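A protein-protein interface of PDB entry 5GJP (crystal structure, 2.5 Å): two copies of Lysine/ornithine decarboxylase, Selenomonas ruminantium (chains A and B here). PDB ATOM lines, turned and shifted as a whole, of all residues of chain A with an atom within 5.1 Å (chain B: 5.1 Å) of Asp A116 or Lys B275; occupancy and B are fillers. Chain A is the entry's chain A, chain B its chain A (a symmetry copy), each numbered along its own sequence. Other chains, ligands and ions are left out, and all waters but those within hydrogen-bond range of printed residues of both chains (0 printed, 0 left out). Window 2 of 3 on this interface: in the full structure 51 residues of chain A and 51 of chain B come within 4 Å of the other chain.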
ATOM      1  N   PRO A  95       1.660  15.886 -29.326  1.00  0.00           N
ATOM      2  CA  PRO A  95       2.589  15.965 -28.180  1.00  0.00           C
ATOM      3  C   PRO A  95       3.718  14.969 -28.275  1.00  0.00           C
ATOM      4  O   PRO A  95       4.756  15.249 -27.731  1.00  0.00           O
ATOM      5  CB  PRO A  95       1.705  15.633 -26.966  1.00  0.00           C
ATOM      6  CG  PRO A  95       0.305  15.873 -27.438  1.00  0.00           C
ATOM      7  CD  PRO A  95       0.329  15.431 -28.881  1.00  0.00           C
ATOM      8  N   VAL A  96       3.522  13.839 -28.976  1.00  0.00           N
ATOM      9  CA  VAL A  96       4.584  12.837 -29.200  1.00  0.00           C
ATOM     10  C   VAL A  96       4.894  12.611 -30.674  1.00  0.00           C
ATOM     11  O   VAL A  96       4.050  12.086 -31.399  1.00  0.00           O
ATOM     12  CB  VAL A  96       4.188  11.474 -28.597  1.00  0.00           C
ATOM     13  CG1 VAL A  96       5.308  10.443 -28.807  1.00  0.00           C
ATOM     14  CG2 VAL A  96       3.844  11.661 -27.126  1.00  0.00           C
ATOM     15  N   THR A 114       4.107  21.483 -29.548  1.00  0.00           N
ATOM     16  CA  THR A 114       3.531  21.236 -28.234  1.00  0.00           C
ATOM     17  C   THR A 114       4.185  19.991 -27.629  1.00  0.00           C
ATOM     18  O   THR A 114       4.777  19.186 -28.340  1.00  0.00           O
ATOM     19  CB  THR A 114       2.014  21.028 -28.305  1.00  0.00           C
ATOM     20  OG1 THR A 114       1.737  19.759 -28.916  1.00  0.00           O
ATOM     21  CG2 THR A 114       1.386  22.164 -29.086  1.00  0.00           C
ATOM     22  N   PHE A 115       4.164  19.858 -26.317  1.00  0.00           N
ATOM     23  CA  PHE A 115       4.676  18.647 -25.705  1.00  0.00           C
ATOM     24  C   PHE A 115       4.094  18.459 -24.324  1.00  0.00           C
ATOM     25  O   PHE A 115       3.665  19.415 -23.714  1.00  0.00           O
ATOM     26  CB  PHE A 115       6.199  18.668 -25.663  1.00  0.00           C
ATOM     27  CG  PHE A 115       6.760  19.547 -24.598  1.00  0.00           C
ATOM     28  CD1 PHE A 115       6.710  20.913 -24.723  1.00  0.00           C
ATOM     29  CD2 PHE A 115       7.328  19.007 -23.472  1.00  0.00           C
ATOM     30  CE1 PHE A 115       7.219  21.727 -23.746  1.00  0.00           C
ATOM     31  CE2 PHE A 115       7.840  19.818 -22.490  1.00  0.00           C
ATOM     32  CZ  PHE A 115       7.785  21.179 -22.630  1.00  0.00           C
ATOM     33  N   ASP A 116       4.058  17.224 -23.842  1.00  0.00           N
ATOM     34  CA  ASP A 116       3.589  16.955 -22.487  1.00  0.00           C
ATOM     35  C   ASP A 116       4.467  16.043 -21.637  1.00  0.00           C
ATOM     36  O   ASP A 116       4.050  15.609 -20.580  1.00  0.00           O
ATOM     37  CB  ASP A 116       2.157  16.444 -22.508  1.00  0.00           C
ATOM     38  CG  ASP A 116       2.018  15.144 -23.233  1.00  0.00           C
ATOM     39  OD1 ASP A 116       3.031  14.609 -23.710  1.00  0.00           O
ATOM     40  OD2 ASP A 116       0.885  14.651 -23.325  1.00  0.00           O
ATOM     41  N   ASP A 117       5.665  15.725 -22.107  1.00  0.00           N
ATOM     42  CA  ASP A 117       6.540  14.820 -21.381  1.00  0.00           C
ATOM     43  C   ASP A 117       7.993  15.215 -21.422  1.00  0.00           C
ATOM     44  O   ASP A 117       8.458  15.802 -22.379  1.00  0.00           O
ATOM     45  CB  ASP A 117       6.393  13.392 -21.905  1.00  0.00           C
ATOM     46  CG  ASP A 117       7.399  12.430 -21.289  1.00  0.00           C
ATOM     47  OD1 ASP A 117       8.538  12.339 -21.788  1.00  0.00           O
ATOM     48  OD2 ASP A 117       7.053  11.768 -20.303  1.00  0.00           O
ATOM     49  N   PRO A 118       8.742  14.831 -20.412  1.00  0.00           N
ATOM     50  CA  PRO A 118      10.170  15.115 -20.401  1.00  0.00           C
ATOM     51  C   PRO A 118      10.886  14.428 -21.544  1.00  0.00           C
ATOM     52  O   PRO A 118      11.802  14.992 -22.090  1.00  0.00           O
ATOM     53  CB  PRO A 118      10.624  14.552 -19.066  1.00  0.00           C
ATOM     54  CG  PRO A 118       9.425  14.616 -18.213  1.00  0.00           C
ATOM     55  CD  PRO A 118       8.276  14.326 -19.119  1.00  0.00           C
ATOM     56  N   VAL A 135       3.673  23.848 -23.442  1.00  0.00           N
ATOM     57  CA  VAL A 135       3.362  22.664 -22.678  1.00  0.00           C
ATOM     58  C   VAL A 135       1.870  22.424 -22.670  1.00  0.00           C
ATOM     59  O   VAL A 135       1.079  23.291 -22.298  1.00  0.00           O
ATOM     60  CB  VAL A 135       3.966  22.674 -21.244  1.00  0.00           C
ATOM     61  CG1 VAL A 135       3.323  23.725 -20.320  1.00  0.00           C
ATOM     62  CG2 VAL A 135       3.884  21.284 -20.641  1.00  0.00           C
ATOM     63  N   ARG A 136       1.488  21.227 -23.074  1.00  0.00           N
ATOM     64  CA  ARG A 136       0.129  20.773 -22.881  1.00  0.00           C
ATOM     65  C   ARG A 136      -0.214  20.252 -21.455  1.00  0.00           C
ATOM     66  O   ARG A 136       0.380  19.292 -20.956  1.00  0.00           O
ATOM     67  CB  ARG A 136      -0.152  19.686 -23.883  1.00  0.00           C
ATOM     68  CG  ARG A 136      -1.615  19.308 -23.899  1.00  0.00           C
ATOM     69  CD  ARG A 136      -2.048  18.927 -25.288  1.00  0.00           C
ATOM     70  NE  ARG A 136      -3.307  18.220 -25.201  1.00  0.00           N
ATOM     71  CZ  ARG A 136      -3.800  17.446 -26.150  1.00  0.00           C
ATOM     72  NH1 ARG A 136      -3.135  17.245 -27.294  1.00  0.00           N
ATOM     73  NH2 ARG A 136      -4.961  16.848 -25.936  1.00  0.00           N
ATOM     74  N   LYS A 151      -4.462   9.906 -22.005  1.00  0.00           N
ATOM     75  CA  LYS A 151      -3.375   9.723 -22.954  1.00  0.00           C
ATOM     76  C   LYS A 151      -2.493  10.959 -23.141  1.00  0.00           C
ATOM     77  O   LYS A 151      -1.302  10.847 -23.360  1.00  0.00           O
ATOM     78  CB  LYS A 151      -3.910   9.266 -24.305  1.00  0.00           C
ATOM     79  CG  LYS A 151      -2.825   9.051 -25.337  1.00  0.00           C
ATOM     80  CD  LYS A 151      -3.305   8.167 -26.460  1.00  0.00           C
ATOM     81  CE  LYS A 151      -2.618   8.536 -27.748  1.00  0.00           C
ATOM     82  NZ  LYS A 151      -1.311   7.861 -27.847  1.00  0.00           N
ATOM     83  N   PHE A 152      -3.102  12.133 -23.107  1.00  0.00           N
ATOM     84  CA  PHE A 152      -2.377  13.365 -23.355  1.00  0.00           C
ATOM     85  C   PHE A 152      -2.462  14.337 -22.197  1.00  0.00           C
ATOM     86  O   PHE A 152      -3.425  14.362 -21.455  1.00  0.00           O
ATOM     87  CB  PHE A 152      -2.908  14.073 -24.602  1.00  0.00           C
ATOM     88  CG  PHE A 152      -3.005  13.201 -25.811  1.00  0.00           C
ATOM     89  CD1 PHE A 152      -1.900  12.955 -26.593  1.00  0.00           C
ATOM     90  CD2 PHE A 152      -4.216  12.652 -26.183  1.00  0.00           C
ATOM     91  CE1 PHE A 152      -1.990  12.165 -27.709  1.00  0.00           C
ATOM     92  CE2 PHE A 152      -4.314  11.861 -27.301  1.00  0.00           C
ATOM     93  CZ  PHE A 152      -3.196  11.616 -28.062  1.00  0.00           C
ATOM     94  N   GLY A 153      -1.430  15.151 -22.075  1.00  0.00           N
ATOM     95  CA  GLY A 153      -1.418  16.269 -21.161  1.00  0.00           C
ATOM     96  C   GLY A 153      -0.670  16.008 -19.881  1.00  0.00           C
ATOM     97  O   GLY A 153      -0.816  14.973 -19.264  1.00  0.00           O
ATOM     98  N   ALA A 154       0.119  16.981 -19.468  1.00  0.00           N
ATOM     99  CA  ALA A 154       0.927  16.827 -18.290  1.00  0.00           C
ATOM    100  C   ALA A 154       0.126  17.268 -17.102  1.00  0.00           C
ATOM    101  O   ALA A 154      -0.727  18.124 -17.215  1.00  0.00           O
ATOM    102  CB  ALA A 154       2.183  17.656 -18.411  1.00  0.00           C
ATOM    103  N   GLU A 158       3.450  19.581 -12.964  1.00  0.00           N
ATOM    104  CA  GLU A 158       4.650  19.306 -13.746  1.00  0.00           C
ATOM    105  C   GLU A 158       4.913  20.424 -14.728  1.00  0.00           C
ATOM    106  O   GLU A 158       6.069  20.619 -15.139  1.00  0.00           O
ATOM    107  CB  GLU A 158       4.517  17.989 -14.521  1.00  0.00           C
ATOM    108  CG  GLU A 158       5.020  16.733 -13.816  1.00  0.00           C
ATOM    109  CD  GLU A 158       5.611  15.728 -14.815  1.00  0.00           C
ATOM    110  OE1 GLU A 158       4.828  15.155 -15.614  1.00  0.00           O
ATOM    111  OE2 GLU A 158       6.862  15.531 -14.816  1.00  0.00           O
ATOM    112  N   LEU A 162       8.333  21.263 -16.632  1.00  0.00           N
ATOM    113  CA  LEU A 162       8.565  20.865 -18.036  1.00  0.00           C
ATOM    114  C   LEU A 162       9.025  22.023 -18.917  1.00  0.00           C
ATOM    115  O   LEU A 162       9.849  21.819 -19.792  1.00  0.00           O
ATOM    116  CB  LEU A 162       7.336  20.197 -18.661  1.00  0.00           C
ATOM    117  CG  LEU A 162       7.020  18.794 -18.157  1.00  0.00           C
ATOM    118  CD1 LEU A 162       5.629  18.405 -18.622  1.00  0.00           C
ATOM    119  CD2 LEU A 162       8.052  17.796 -18.643  1.00  0.00           C
ATOM    120  N   GLY B 273       7.697   7.456 -27.732  1.00  0.00           N
ATOM    121  CA  GLY B 273       7.559   8.306 -26.537  1.00  0.00           C
ATOM    122  C   GLY B 273       7.306   7.469 -25.299  1.00  0.00           C
ATOM    123  O   GLY B 273       6.705   6.383 -25.377  1.00  0.00           O
ATOM    124  N   THR B 274       7.728   7.961 -24.150  1.00  0.00           N
ATOM    125  CA  THR B 274       7.461   7.266 -22.898  1.00  0.00           C
ATOM    126  C   THR B 274       6.704   8.178 -21.965  1.00  0.00           C
ATOM    127  O   THR B 274       6.806   9.377 -22.059  1.00  0.00           O
ATOM    128  CB  THR B 274       8.734   6.763 -22.199  1.00  0.00           C
ATOM    129  OG1 THR B 274       9.636   7.847 -21.995  1.00  0.00           O
ATOM    130  CG2 THR B 274       9.412   5.702 -23.013  1.00  0.00           C
ATOM    131  N   LYS B 275       5.894   7.595 -21.103  1.00  0.00           N
ATOM    132  CA  LYS B 275       5.172   8.354 -20.105  1.00  0.00           C
ATOM    133  C   LYS B 275       5.308   7.707 -18.748  1.00  0.00           C
ATOM    134  O   LYS B 275       4.396   7.055 -18.275  1.00  0.00           O
ATOM    135  CB  LYS B 275       3.700   8.488 -20.477  1.00  0.00           C
ATOM    136  CG  LYS B 275       3.315   9.846 -21.015  1.00  0.00           C
ATOM    137  CD  LYS B 275       2.008   9.779 -21.775  1.00  0.00           C
ATOM    138  CE  LYS B 275       2.152  10.339 -23.178  1.00  0.00           C
ATOM    139  NZ  LYS B 275       3.206  11.378 -23.271  1.00  0.00           N
ATOM    140  N   THR B 276       6.462   7.896 -18.133  1.00  0.00           N
ATOM    141  CA  THR B 276       6.704   7.342 -16.818  1.00  0.00           C
ATOM    142  C   THR B 276       6.162   8.266 -15.743  1.00  0.00           C
ATOM    143  O   THR B 276       6.888   8.747 -14.890  1.00  0.00           O
ATOM    144  CB  THR B 276       8.203   7.115 -16.594  1.00  0.00           C
ATOM    145  OG1 THR B 276       8.738   6.327 -17.665  1.00  0.00           O
ATOM    146  CG2 THR B 276       8.416   6.412 -15.288  1.00  0.00           C
ATOM    147  N   ARG B 277       4.859   8.492 -15.785  1.00  0.00           N
ATOM    148  CA  ARG B 277       4.160   9.209 -14.731  1.00  0.00           C
ATOM    149  C   ARG B 277       3.998   8.350 -13.482  1.00  0.00           C
ATOM    150  O   ARG B 277       4.145   8.822 -12.364  1.00  0.00           O
ATOM    151  CB  ARG B 277       2.791   9.672 -15.237  1.00  0.00           C
ATOM    152  CG  ARG B 277       2.643  11.173 -15.444  1.00  0.00           C
ATOM    153  CD  ARG B 277       1.678  11.524 -16.576  1.00  0.00           C
ATOM    154  NE  ARG B 277       0.812  10.407 -16.965  1.00  0.00           N
ATOM    155  CZ  ARG B 277      -0.166  10.473 -17.864  1.00  0.00           C
ATOM    156  NH1 ARG B 277      -0.433  11.609 -18.492  1.00  0.00           N
ATOM    157  NH2 ARG B 277      -0.881   9.393 -18.134  1.00  0.00           N
ATOM    158  N   GLY B 278       3.676   7.079 -13.695  1.00  0.00           N
ATOM    159  CA  GLY B 278       3.370   6.154 -12.621  1.00  0.00           C
ATOM    160  C   GLY B 278       1.880   6.198 -12.372  1.00  0.00           C
ATOM    161  O   GLY B 278       1.252   7.188 -12.716  1.00  0.00           O
ATOM    162  N   GLN B 280       1.663   3.189 -13.709  1.00  0.00           N
ATOM    163  CA  GLN B 280       1.920   2.406 -14.905  1.00  0.00           C
ATOM    164  C   GLN B 280       2.593   3.211 -16.007  1.00  0.00           C
ATOM    165  O   GLN B 280       2.141   4.288 -16.349  1.00  0.00           O
ATOM    166  CB  GLN B 280       0.593   1.877 -15.424  1.00  0.00           C
ATOM    167  CG  GLN B 280       0.661   0.507 -16.050  1.00  0.00           C
ATOM    168  CD  GLN B 280      -0.701  -0.002 -16.417  1.00  0.00           C
ATOM    169  OE1 GLN B 280      -1.464  -0.409 -15.566  1.00  0.00           O
ATOM    170  NE2 GLN B 280      -1.016   0.030 -17.686  1.00  0.00           N
ATOM    171  N   PRO B 281       3.670   2.688 -16.569  1.00  0.00           N
ATOM    172  CA  PRO B 281       4.316   3.352 -17.702  1.00  0.00           C
ATOM    173  C   PRO B 281       3.544   3.242 -19.019  1.00  0.00           C
ATOM    174  O   PRO B 281       3.041   2.189 -19.342  1.00  0.00           O
ATOM    175  CB  PRO B 281       5.666   2.639 -17.808  1.00  0.00           C
ATOM    176  CG  PRO B 281       5.523   1.398 -17.023  1.00  0.00           C
ATOM    177  CD  PRO B 281       4.547   1.697 -15.946  1.00  0.00           C
ATOM    178  N   TRP B 282       3.485   4.324 -19.777  1.00  0.00           N
ATOM    179  CA  TRP B 282       2.866   4.317 -21.088  1.00  0.00           C
ATOM    180  C   TRP B 282       3.952   4.320 -22.113  1.00  0.00           C
ATOM    181  O   TRP B 282       4.869   5.138 -22.031  1.00  0.00           O
ATOM    182  CB  TRP B 282       2.004   5.545 -21.319  1.00  0.00           C
ATOM    183  CG  TRP B 282       0.704   5.496 -20.696  1.00  0.00           C
ATOM    184  CD1 TRP B 282       0.444   5.255 -19.392  1.00  0.00           C
ATOM    185  CD2 TRP B 282      -0.545   5.730 -21.328  1.00  0.00           C
ATOM    186  NE1 TRP B 282      -0.904   5.319 -19.162  1.00  0.00           N
ATOM    187  CE2 TRP B 282      -1.540   5.610 -20.334  1.00  0.00           C
ATOM    188  CE3 TRP B 282      -0.930   6.023 -22.645  1.00  0.00           C
ATOM    189  CZ2 TRP B 282      -2.890   5.762 -20.603  1.00  0.00           C
ATOM    190  CZ3 TRP B 282      -2.287   6.195 -22.914  1.00  0.00           C
ATOM    191  CH2 TRP B 282      -3.251   6.060 -21.894  1.00  0.00           C
ATOM    192  N   TYR B 283       3.857   3.396 -23.060  1.00  0.00           N
ATOM    193  CA  TYR B 283       4.756   3.368 -24.196  1.00  0.00           C
ATOM    194  C   TYR B 283       3.934   3.742 -25.398  1.00  0.00           C
ATOM    195  O   TYR B 283       2.930   3.076 -25.691  1.00  0.00           O
ATOM    196  CB  TYR B 283       5.376   1.996 -24.360  1.00  0.00           C
ATOM    197  CG  TYR B 283       6.197   1.629 -23.163  1.00  0.00           C
ATOM    198  CD1 TYR B 283       7.337   2.348 -22.844  1.00  0.00           C
ATOM    199  CD2 TYR B 283       5.822   0.579 -22.322  1.00  0.00           C
ATOM    200  CE1 TYR B 283       8.089   2.032 -21.724  1.00  0.00           C
ATOM    201  CE2 TYR B 283       6.567   0.252 -21.217  1.00  0.00           C
ATOM    202  CZ  TYR B 283       7.703   0.986 -20.918  1.00  0.00           C
ATOM    203  OH  TYR B 283       8.474   0.664 -19.818  1.00  0.00           O
ATOM    204  N   ILE B 284       4.326   4.843 -26.048  1.00  0.00           N
ATOM    205  CA  ILE B 284       3.698   5.256 -27.293  1.00  0.00           C
ATOM    206  C   ILE B 284       4.460   4.690 -28.491  1.00  0.00           C
ATOM    207  O   ILE B 284       5.650   4.961 -28.645  1.00  0.00           O
ATOM    208  CB  ILE B 284       3.623   6.786 -27.415  1.00  0.00           C
ATOM    209  CG1 ILE B 284       2.891   7.389 -26.217  1.00  0.00           C
ATOM    210  CG2 ILE B 284       2.900   7.192 -28.703  1.00  0.00           C
ATOM    211  CD1 ILE B 284       1.446   6.943 -26.079  1.00  0.00           C
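The backbone carbonyl oxygen of Thr B274 lies close to the side-chain carboxylate of Asp A117, at 3.0 Å. The side-chain amino group (NZ) of Lys B275 is in salt-bridge range of the side-chain carboxylate (OD1) of Asp A116, 3.3 Å away. NH1 of Arg B277 sits at hydrogen-bond distance from O of Gly A153, at 3.5 Å.
Asp A116 touches just one residue of chain B: Lys B275. Of the printed residues of chain A, Lys B275 touches Val A96 (3.9 Å), Asp A116 (3.3 Å), Asp A117 (3.9 Å) and Lys A151 (3.5 Å). Printed residues of chain A within 4 Å of Arg B277: Gly A153 (3.5 Å). Of the printed residues of chain A, Ile B284 touches Lys A151. Printed residues of chain B within 4 Å of Val A96: Gly B273 (3.8 Å) and Lys B275 (3.9 Å). Printed residues of chain B within 4 Å of Lys A151: Lys B275, Trp B282 and Ile B284. Of the printed residues of chain B, Asp A117 touches Thr B274 (3.0 Å) and Lys B275 (3.9 Å). Thr A114 touches none of the printed residues of chain B. The nearest printed residue of chain A that does not touch Lys B275 is Phe A152 (5.4 Å).
No position is printed for both chains.
The backbone carbonyl oxygen of Trp B282 is in hydrogen-bond range of the backbone NH of Lys B275 (2.8 Å). The backbone carbonyl oxygen (O) of Gly B273 sits at hydrogen-bond distance from the backbone NH (N) of Ile B284, at 2.9 Å. OD2 of Asp A116 sits at hydrogen-bond distance from N of Gly A153, at 2.7 Å.
Gly B273 touches Val A96 (CA to CG1, 3.8 Å). CG2 of Val A96 touches NZ of Lys B275, at 3.9 Å. Lys B275 touches Asp A117. Lys B275 touches Lys A151. CZ3 of Trp B282 touches CA of Lys A151, 3.7 Å away. NZ of Lys A151 touches CD1 of Ile B284, at 3.4 Å.
Hydrophobic or aromatic side chains of chain A within 4 Å of the printed part of chain B: Val A96. Of the 11 printed residues of chain B, 6 touch a printed residue of chain A. Printed residues of chain B that touch a printed residue of chain A: Gly B273, Thr B274, Lys B275, Arg B277, Trp B282 and Ile B284. Along chain B the printed residues that touch a printed residue of chain A span positions 273 to 284. Among the printed residues, Asp or Glu carboxylates within 4 Å of a Lys or Arg side-chain nitrogen of the other chain: Asp A116 with Lys B275.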
